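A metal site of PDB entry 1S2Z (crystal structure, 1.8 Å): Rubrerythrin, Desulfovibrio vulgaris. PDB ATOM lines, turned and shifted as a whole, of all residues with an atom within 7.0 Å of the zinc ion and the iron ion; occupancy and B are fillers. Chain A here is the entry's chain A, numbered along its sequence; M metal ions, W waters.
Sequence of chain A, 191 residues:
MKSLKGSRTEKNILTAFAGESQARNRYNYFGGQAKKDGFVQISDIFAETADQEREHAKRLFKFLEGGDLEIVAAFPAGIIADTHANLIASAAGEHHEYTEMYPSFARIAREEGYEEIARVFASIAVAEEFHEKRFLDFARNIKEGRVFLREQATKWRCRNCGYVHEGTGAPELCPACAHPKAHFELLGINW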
ATOM      1  N   GLU A  20       7.683 -15.750   7.079  1.00  0.00           N
ATOM      2  CA  GLU A  20       6.230 -15.822   7.144  1.00  0.00           C
ATOM      3  C   GLU A  20       5.623 -15.468   5.798  1.00  0.00           C
ATOM      4  O   GLU A  20       4.599 -16.016   5.400  1.00  0.00           O
ATOM      5  CB  GLU A  20       5.700 -14.887   8.229  1.00  0.00           C
ATOM      6  CG  GLU A  20       6.113 -15.286   9.636  1.00  0.00           C
ATOM      7  CD  GLU A  20       5.448 -16.564  10.095  1.00  0.00           C
ATOM      8  OE1 GLU A  20       5.681 -17.630   9.490  1.00  0.00           O
ATOM      9  OE2 GLU A  20       4.686 -16.498  11.078  1.00  0.00           O
ATOM     10  N   ALA A  23       5.945 -18.397   3.578  1.00  0.00           N
ATOM     11  CA  ALA A  23       5.016 -19.433   4.032  1.00  0.00           C
ATOM     12  C   ALA A  23       3.620 -19.159   3.481  1.00  0.00           C
ATOM     13  O   ALA A  23       2.915 -20.080   3.061  1.00  0.00           O
ATOM     14  CB  ALA A  23       4.991 -19.495   5.557  1.00  0.00           C
ATOM     15  N   TYR A  27       1.753 -21.969   1.233  1.00  0.00           N
ATOM     16  CA  TYR A  27       0.472 -22.523   1.653  1.00  0.00           C
ATOM     17  C   TYR A  27      -0.638 -22.287   0.629  1.00  0.00           C
ATOM     18  O   TYR A  27      -1.493 -23.158   0.431  1.00  0.00           O
ATOM     19  CB  TYR A  27       0.075 -21.954   3.029  1.00  0.00           C
ATOM     20  CG  TYR A  27       0.996 -22.409   4.148  1.00  0.00           C
ATOM     21  CD1 TYR A  27       1.930 -23.434   3.945  1.00  0.00           C
ATOM     22  CD2 TYR A  27       0.944 -21.821   5.411  1.00  0.00           C
ATOM     23  CE1 TYR A  27       2.774 -23.858   4.984  1.00  0.00           C
ATOM     24  CE2 TYR A  27       1.778 -22.231   6.448  1.00  0.00           C
ATOM     25  CZ  TYR A  27       2.696 -23.250   6.220  1.00  0.00           C
ATOM     26  OH  TYR A  27       3.522 -23.661   7.241  1.00  0.00           O
ATOM     27  N   THR A  49      -4.675 -21.035   6.622  1.00  0.00           N
ATOM     28  CA  THR A  49      -3.378 -20.941   7.269  1.00  0.00           C
ATOM     29  C   THR A  49      -2.552 -19.848   6.592  1.00  0.00           C
ATOM     30  O   THR A  49      -1.860 -19.089   7.256  1.00  0.00           O
ATOM     31  CB  THR A  49      -2.608 -22.276   7.194  1.00  0.00           C
ATOM     32  OG1 THR A  49      -3.452 -23.331   7.686  1.00  0.00           O
ATOM     33  CG2 THR A  49      -1.348 -22.211   8.052  1.00  0.00           C
ATOM     34  N   GLN A  52      -3.570 -16.596   7.856  1.00  0.00           N
ATOM     35  CA  GLN A  52      -3.109 -16.382   9.212  1.00  0.00           C
ATOM     36  C   GLN A  52      -1.617 -16.038   9.210  1.00  0.00           C
ATOM     37  O   GLN A  52      -1.169 -15.253  10.046  1.00  0.00           O
ATOM     38  CB  GLN A  52      -3.431 -17.594  10.087  1.00  0.00           C
ATOM     39  CG  GLN A  52      -4.952 -17.836  10.136  1.00  0.00           C
ATOM     40  CD  GLN A  52      -5.378 -18.937  11.079  1.00  0.00           C
ATOM     41  OE1 GLN A  52      -4.655 -19.898  11.317  1.00  0.00           O
ATOM     42  NE2 GLN A  52      -6.601 -18.811  11.617  1.00  0.00           N
ATOM     43  N   GLU A  53      -0.861 -16.597   8.270  1.00  0.00           N
ATOM     44  CA  GLU A  53       0.557 -16.273   8.170  1.00  0.00           C
ATOM     45  C   GLU A  53       0.678 -14.812   7.740  1.00  0.00           C
ATOM     46  O   GLU A  53       1.612 -14.107   8.127  1.00  0.00           O
ATOM     47  CB  GLU A  53       1.281 -17.155   7.137  1.00  0.00           C
ATOM     48  CG  GLU A  53       1.239 -18.654   7.410  1.00  0.00           C
ATOM     49  CD  GLU A  53       1.716 -19.026   8.798  1.00  0.00           C
ATOM     50  OE1 GLU A  53       2.546 -18.288   9.373  1.00  0.00           O
ATOM     51  OE2 GLU A  53       1.272 -20.075   9.324  1.00  0.00           O
ATOM     52  N   ARG A  54      -0.275 -14.353   6.917  1.00  0.00           N
ATOM     53  CA  ARG A  54      -0.295 -12.962   6.481  1.00  0.00           C
ATOM     54  C   ARG A  54      -0.433 -12.072   7.704  1.00  0.00           C
ATOM     55  O   ARG A  54       0.196 -11.015   7.799  1.00  0.00           O
ATOM     56  CB  ARG A  54      -1.483 -12.714   5.551  1.00  0.00           C
ATOM     57  CG  ARG A  54      -1.732 -11.238   5.206  1.00  0.00           C
ATOM     58  CD  ARG A  54      -3.116 -11.075   4.585  1.00  0.00           C
ATOM     59  NE  ARG A  54      -4.156 -11.428   5.538  1.00  0.00           N
ATOM     60  CZ  ARG A  54      -5.376 -11.858   5.213  1.00  0.00           C
ATOM     61  NH1 ARG A  54      -5.721 -11.996   3.945  1.00  0.00           N
ATOM     62  NH2 ARG A  54      -6.237 -12.168   6.181  1.00  0.00           N
ATOM     63  N   GLU A  55      -1.260 -12.511   8.657  1.00  0.00           N
ATOM     64  CA  GLU A  55      -1.487 -11.734   9.870  1.00  0.00           C
ATOM     65  C   GLU A  55      -0.297 -11.789  10.839  1.00  0.00           C
ATOM     66  O   GLU A  55      -0.026 -10.807  11.524  1.00  0.00           O
ATOM     67  CB  GLU A  55      -2.782 -12.215  10.542  1.00  0.00           C
ATOM     68  CG  GLU A  55      -4.022 -11.969   9.682  1.00  0.00           C
ATOM     69  CD  GLU A  55      -4.206 -10.502   9.313  1.00  0.00           C
ATOM     70  OE1 GLU A  55      -4.149  -9.653  10.234  1.00  0.00           O
ATOM     71  OE2 GLU A  55      -4.404 -10.191   8.122  1.00  0.00           O
ATOM     72  N   HIS A  56       0.399 -12.910  10.889  1.00  0.00           N
ATOM     73  CA  HIS A  56       1.588 -12.993  11.751  1.00  0.00           C
ATOM     74  C   HIS A  56       2.607 -12.000  11.193  1.00  0.00           C
ATOM     75  O   HIS A  56       3.235 -11.236  11.932  1.00  0.00           O
ATOM     76  CB  HIS A  56       2.202 -14.396  11.696  1.00  0.00           C
ATOM     77  CG  HIS A  56       1.345 -15.464  12.323  1.00  0.00           C
ATOM     78  ND1 HIS A  56       1.626 -16.806  12.197  1.00  0.00           N
ATOM     79  CD2 HIS A  56       0.234 -15.374  13.092  1.00  0.00           C
ATOM     80  CE1 HIS A  56       0.720 -17.496  12.857  1.00  0.00           C
ATOM     81  NE2 HIS A  56      -0.132 -16.656  13.410  1.00  0.00           N
ATOM     82  N   ALA A  57       2.748 -12.018   9.874  1.00  0.00           N
ATOM     83  CA  ALA A  57       3.687 -11.131   9.193  1.00  0.00           C
ATOM     84  C   ALA A  57       3.307  -9.662   9.415  1.00  0.00           C
ATOM     85  O   ALA A  57       4.172  -8.820   9.616  1.00  0.00           O
ATOM     86  CB  ALA A  57       3.719 -11.449   7.693  1.00  0.00           C
ATOM     87  N   LEU A  60       4.327  -8.466  12.873  1.00  0.00           N
ATOM     88  CA  LEU A  60       5.777  -8.298  12.882  1.00  0.00           C
ATOM     89  C   LEU A  60       6.203  -7.052  12.109  1.00  0.00           C
ATOM     90  O   LEU A  60       7.019  -6.270  12.586  1.00  0.00           O
ATOM     91  CB  LEU A  60       6.467  -9.522  12.281  1.00  0.00           C
ATOM     92  CG  LEU A  60       6.296 -10.842  13.046  1.00  0.00           C
ATOM     93  CD1 LEU A  60       6.789 -11.996  12.176  1.00  0.00           C
ATOM     94  CD2 LEU A  60       7.071 -10.774  14.351  1.00  0.00           C
ATOM     95  N   SER A  90       4.915 -28.782   5.217  1.00  0.00           N
ATOM     96  CA  SER A  90       4.349 -27.644   5.923  1.00  0.00           C
ATOM     97  C   SER A  90       4.470 -27.828   7.431  1.00  0.00           C
ATOM     98  O   SER A  90       4.805 -26.887   8.158  1.00  0.00           O
ATOM     99  CB  SER A  90       2.885 -27.438   5.529  1.00  0.00           C
ATOM    100  OG  SER A  90       2.770 -27.089   4.156  1.00  0.00           O
ATOM    101  N   GLY A  93       7.927 -27.179   8.598  1.00  0.00           N
ATOM    102  CA  GLY A  93       8.207 -25.753   8.652  1.00  0.00           C
ATOM    103  C   GLY A  93       7.643 -25.154   9.932  1.00  0.00           C
ATOM    104  O   GLY A  93       8.312 -24.373  10.613  1.00  0.00           O
ATOM    105  N   GLU A  94       6.403 -25.509  10.239  1.00  0.00           N
ATOM    106  CA  GLU A  94       5.760 -25.012  11.454  1.00  0.00           C
ATOM    107  C   GLU A  94       6.553 -25.489  12.667  1.00  0.00           C
ATOM    108  O   GLU A  94       6.769 -24.731  13.615  1.00  0.00           O
ATOM    109  CB  GLU A  94       4.323 -25.535  11.550  1.00  0.00           C
ATOM    110  CG  GLU A  94       3.383 -25.102  10.421  1.00  0.00           C
ATOM    111  CD  GLU A  94       2.912 -23.654  10.528  1.00  0.00           C
ATOM    112  OE1 GLU A  94       3.117 -23.030  11.597  1.00  0.00           O
ATOM    113  OE2 GLU A  94       2.320 -23.142   9.557  1.00  0.00           O
ATOM    114  N   GLU A  97       9.585 -23.432  13.276  1.00  0.00           N
ATOM    115  CA  GLU A  97       9.157 -22.131  13.774  1.00  0.00           C
ATOM    116  C   GLU A  97       8.766 -22.081  15.241  1.00  0.00           C
ATOM    117  O   GLU A  97       9.164 -21.161  15.959  1.00  0.00           O
ATOM    118  CB  GLU A  97       8.006 -21.594  12.918  1.00  0.00           C
ATOM    119  CG  GLU A  97       8.459 -21.121  11.551  1.00  0.00           C
ATOM    120  CD  GLU A  97       7.302 -20.852  10.618  1.00  0.00           C
ATOM    121  OE1 GLU A  97       6.353 -20.147  11.032  1.00  0.00           O
ATOM    122  OE2 GLU A  97       7.346 -21.334   9.462  1.00  0.00           O
ATOM    123  N   TYR A 102      10.979 -19.047  16.788  1.00  0.00           N
ATOM    124  CA  TYR A 102      10.289 -18.123  17.688  1.00  0.00           C
ATOM    125  C   TYR A 102      10.777 -18.159  19.121  1.00  0.00           C
ATOM    126  O   TYR A 102      10.947 -17.102  19.747  1.00  0.00           O
ATOM    127  CB  TYR A 102       8.764 -18.331  17.589  1.00  0.00           C
ATOM    128  CG  TYR A 102       8.176 -17.659  16.357  1.00  0.00           C
ATOM    129  CD1 TYR A 102       8.397 -16.301  16.110  1.00  0.00           C
ATOM    130  CD2 TYR A 102       7.441 -18.384  15.417  1.00  0.00           C
ATOM    131  CE1 TYR A 102       7.894 -15.673  14.975  1.00  0.00           C
ATOM    132  CE2 TYR A 102       6.930 -17.763  14.273  1.00  0.00           C
ATOM    133  CZ  TYR A 102       7.164 -16.410  14.065  1.00  0.00           C
ATOM    134  OH  TYR A 102       6.670 -15.775  12.938  1.00  0.00           O
ATOM    135  N   ILE A 124       2.871 -16.079  18.767  1.00  0.00           N
ATOM    136  CA  ILE A 124       2.788 -16.573  17.402  1.00  0.00           C
ATOM    137  C   ILE A 124       3.176 -18.044  17.368  1.00  0.00           C
ATOM    138  O   ILE A 124       2.587 -18.836  16.638  1.00  0.00           O
ATOM    139  CB  ILE A 124       3.713 -15.766  16.458  1.00  0.00           C
ATOM    140  CG1 ILE A 124       3.199 -14.324  16.349  1.00  0.00           C
ATOM    141  CG2 ILE A 124       3.737 -16.410  15.071  1.00  0.00           C
ATOM    142  CD1 ILE A 124       4.094 -13.417  15.515  1.00  0.00           C
ATOM    143  N   ALA A 127       0.336 -20.333  17.859  1.00  0.00           N
ATOM    144  CA  ALA A 127      -0.478 -20.492  16.667  1.00  0.00           C
ATOM    145  C   ALA A 127       0.150 -21.504  15.719  1.00  0.00           C
ATOM    146  O   ALA A 127      -0.538 -22.342  15.146  1.00  0.00           O
ATOM    147  CB  ALA A 127      -0.622 -19.146  15.953  1.00  0.00           C
ATOM    148  N   GLU A 128       1.476 -21.430  15.567  1.00  0.00           N
ATOM    149  CA  GLU A 128       2.186 -22.340  14.670  1.00  0.00           C
ATOM    150  C   GLU A 128       2.111 -23.792  15.129  1.00  0.00           C
ATOM    151  O   GLU A 128       2.086 -24.713  14.312  1.00  0.00           O
ATOM    152  CB  GLU A 128       3.658 -21.925  14.552  1.00  0.00           C
ATOM    153  CG  GLU A 128       3.875 -20.421  14.381  1.00  0.00           C
ATOM    154  CD  GLU A 128       3.420 -19.877  13.030  1.00  0.00           C
ATOM    155  OE1 GLU A 128       2.365 -20.319  12.518  1.00  0.00           O
ATOM    156  OE2 GLU A 128       4.111 -18.994  12.492  1.00  0.00           O
ATOM    157  N   GLU A 129       2.074 -24.016  16.439  1.00  0.00           N
ATOM    158  CA  GLU A 129       1.993 -25.388  16.927  1.00  0.00           C
ATOM    159  C   GLU A 129       0.654 -26.013  16.528  1.00  0.00           C
ATOM    160  O   GLU A 129       0.588 -27.189  16.180  1.00  0.00           O
ATOM    161  CB  GLU A 129       2.182 -25.453  18.447  1.00  0.00           C
ATOM    162  CG  GLU A 129       2.117 -26.869  19.020  1.00  0.00           C
ATOM    163  CD  GLU A 129       2.860 -27.006  20.339  1.00  0.00           C
ATOM    164  OE1 GLU A 129       3.059 -25.988  21.030  1.00  0.00           O
ATOM    165  OE2 GLU A 129       3.229 -28.149  20.692  1.00  0.00           O
ATOM    166  N   HIS A 131      -1.022 -25.035  13.919  1.00  0.00           N
ATOM    167  CA  HIS A 131      -0.947 -25.131  12.464  1.00  0.00           C
ATOM    168  C   HIS A 131      -0.318 -26.494  12.149  1.00  0.00           C
ATOM    169  O   HIS A 131      -0.810 -27.224  11.273  1.00  0.00           O
ATOM    170  CB  HIS A 131      -0.057 -24.032  11.883  1.00  0.00           C
ATOM    171  CG  HIS A 131      -0.756 -22.712  11.728  1.00  0.00           C
ATOM    172  ND1 HIS A 131      -0.082 -21.554  11.393  1.00  0.00           N
ATOM    173  CD2 HIS A 131      -2.057 -22.377  11.844  1.00  0.00           C
ATOM    174  CE1 HIS A 131      -0.945 -20.554  11.315  1.00  0.00           C
ATOM    175  NE2 HIS A 131      -2.148 -21.026  11.578  1.00  0.00           N
ATOM    176  N   GLU A 132       0.747 -26.833  12.855  1.00  0.00           N
ATOM    177  CA  GLU A 132       1.410 -28.127  12.635  1.00  0.00           C
ATOM    178  C   GLU A 132       0.478 -29.285  12.939  1.00  0.00           C
ATOM    179  O   GLU A 132       0.422 -30.266  12.184  1.00  0.00           O
ATOM    180  CB  GLU A 132       2.672 -28.282  13.487  1.00  0.00           C
ATOM    181  CG  GLU A 132       3.412 -29.595  13.181  1.00  0.00           C
ATOM    182  CD  GLU A 132       4.301 -30.077  14.311  1.00  0.00           C
ATOM    183  OE1 GLU A 132       3.880 -30.002  15.484  1.00  0.00           O
ATOM    184  OE2 GLU A 132       5.410 -30.570  14.020  1.00  0.00           O
ATOM    185  N   PHE A 135      -1.872 -29.871  10.042  1.00  0.00           N
ATOM    186  CA  PHE A 135      -1.172 -30.441   8.906  1.00  0.00           C
ATOM    187  C   PHE A 135      -0.829 -31.911   9.124  1.00  0.00           C
ATOM    188  O   PHE A 135      -1.024 -32.743   8.235  1.00  0.00           O
ATOM    189  CB  PHE A 135       0.099 -29.633   8.591  1.00  0.00           C
ATOM    190  CG  PHE A 135      -0.159 -28.240   8.063  1.00  0.00           C
ATOM    191  CD1 PHE A 135      -1.224 -27.995   7.191  1.00  0.00           C
ATOM    192  CD2 PHE A 135       0.693 -27.191   8.393  1.00  0.00           C
ATOM    193  CE1 PHE A 135      -1.417 -26.710   6.645  1.00  0.00           C
ATOM    194  CE2 PHE A 135       0.508 -25.912   7.856  1.00  0.00           C
ATOM    195  CZ  PHE A 135      -0.546 -25.675   6.979  1.00  0.00           C
HETATM  196 ZN    ZN M   1       3.180 -17.771  11.180  1.00  0.00          ZN
HETATM  197 FE    FE M   2       1.994 -21.319  10.731  1.00  0.00          FE
HETATM  198  O   HOH W   1       4.085 -20.805   9.860  1.00  0.00           O
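OE2 of Glu 20 lies close to OH of Tyr 102 (2.8 Å). The side-chain amide oxygen (OE1) of Gln 52 lies within hydrogen-bond range of a ring nitrogen (NE2) of His 131, 2.8 Å away. The side-chain hydroxyl (OH) of Tyr 27 sits close to the side-chain carboxylate (OE2) of Glu 94. The backbone NH of Tyr 102 lies within hydrogen-bond range of the backbone carbonyl oxygen of Glu 97, 2.9 Å away.
Residues that only touch the zinc ion: Glu 97.
Of the 23 residues printed, 4 come within 4 Å of the iron ion. The nearest printed residue that does not touch the iron ion is Thr 49 (4.4 Å).
The zinc ion is bound by OE2 of Glu 20 (2.0 Å), OE1 of Glu 53 (2.0 Å), OE2 of Glu 128 (2.0 Å) and ND1 of His 56 (2.1 Å). The zinc ion has four donor atoms within binding distance.
The iron ion is bound by OE2 of Glu 53 (2.0 Å), OE1 of Glu 128 (2.1 Å), ND1 of His 131 (2.2 Å), OE2 of Glu 94 (2.2 Å), OE1 of Glu 94 (2.2 Å) and water W1 (2.3 Å). The iron ion has six donor atoms within binding distance.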
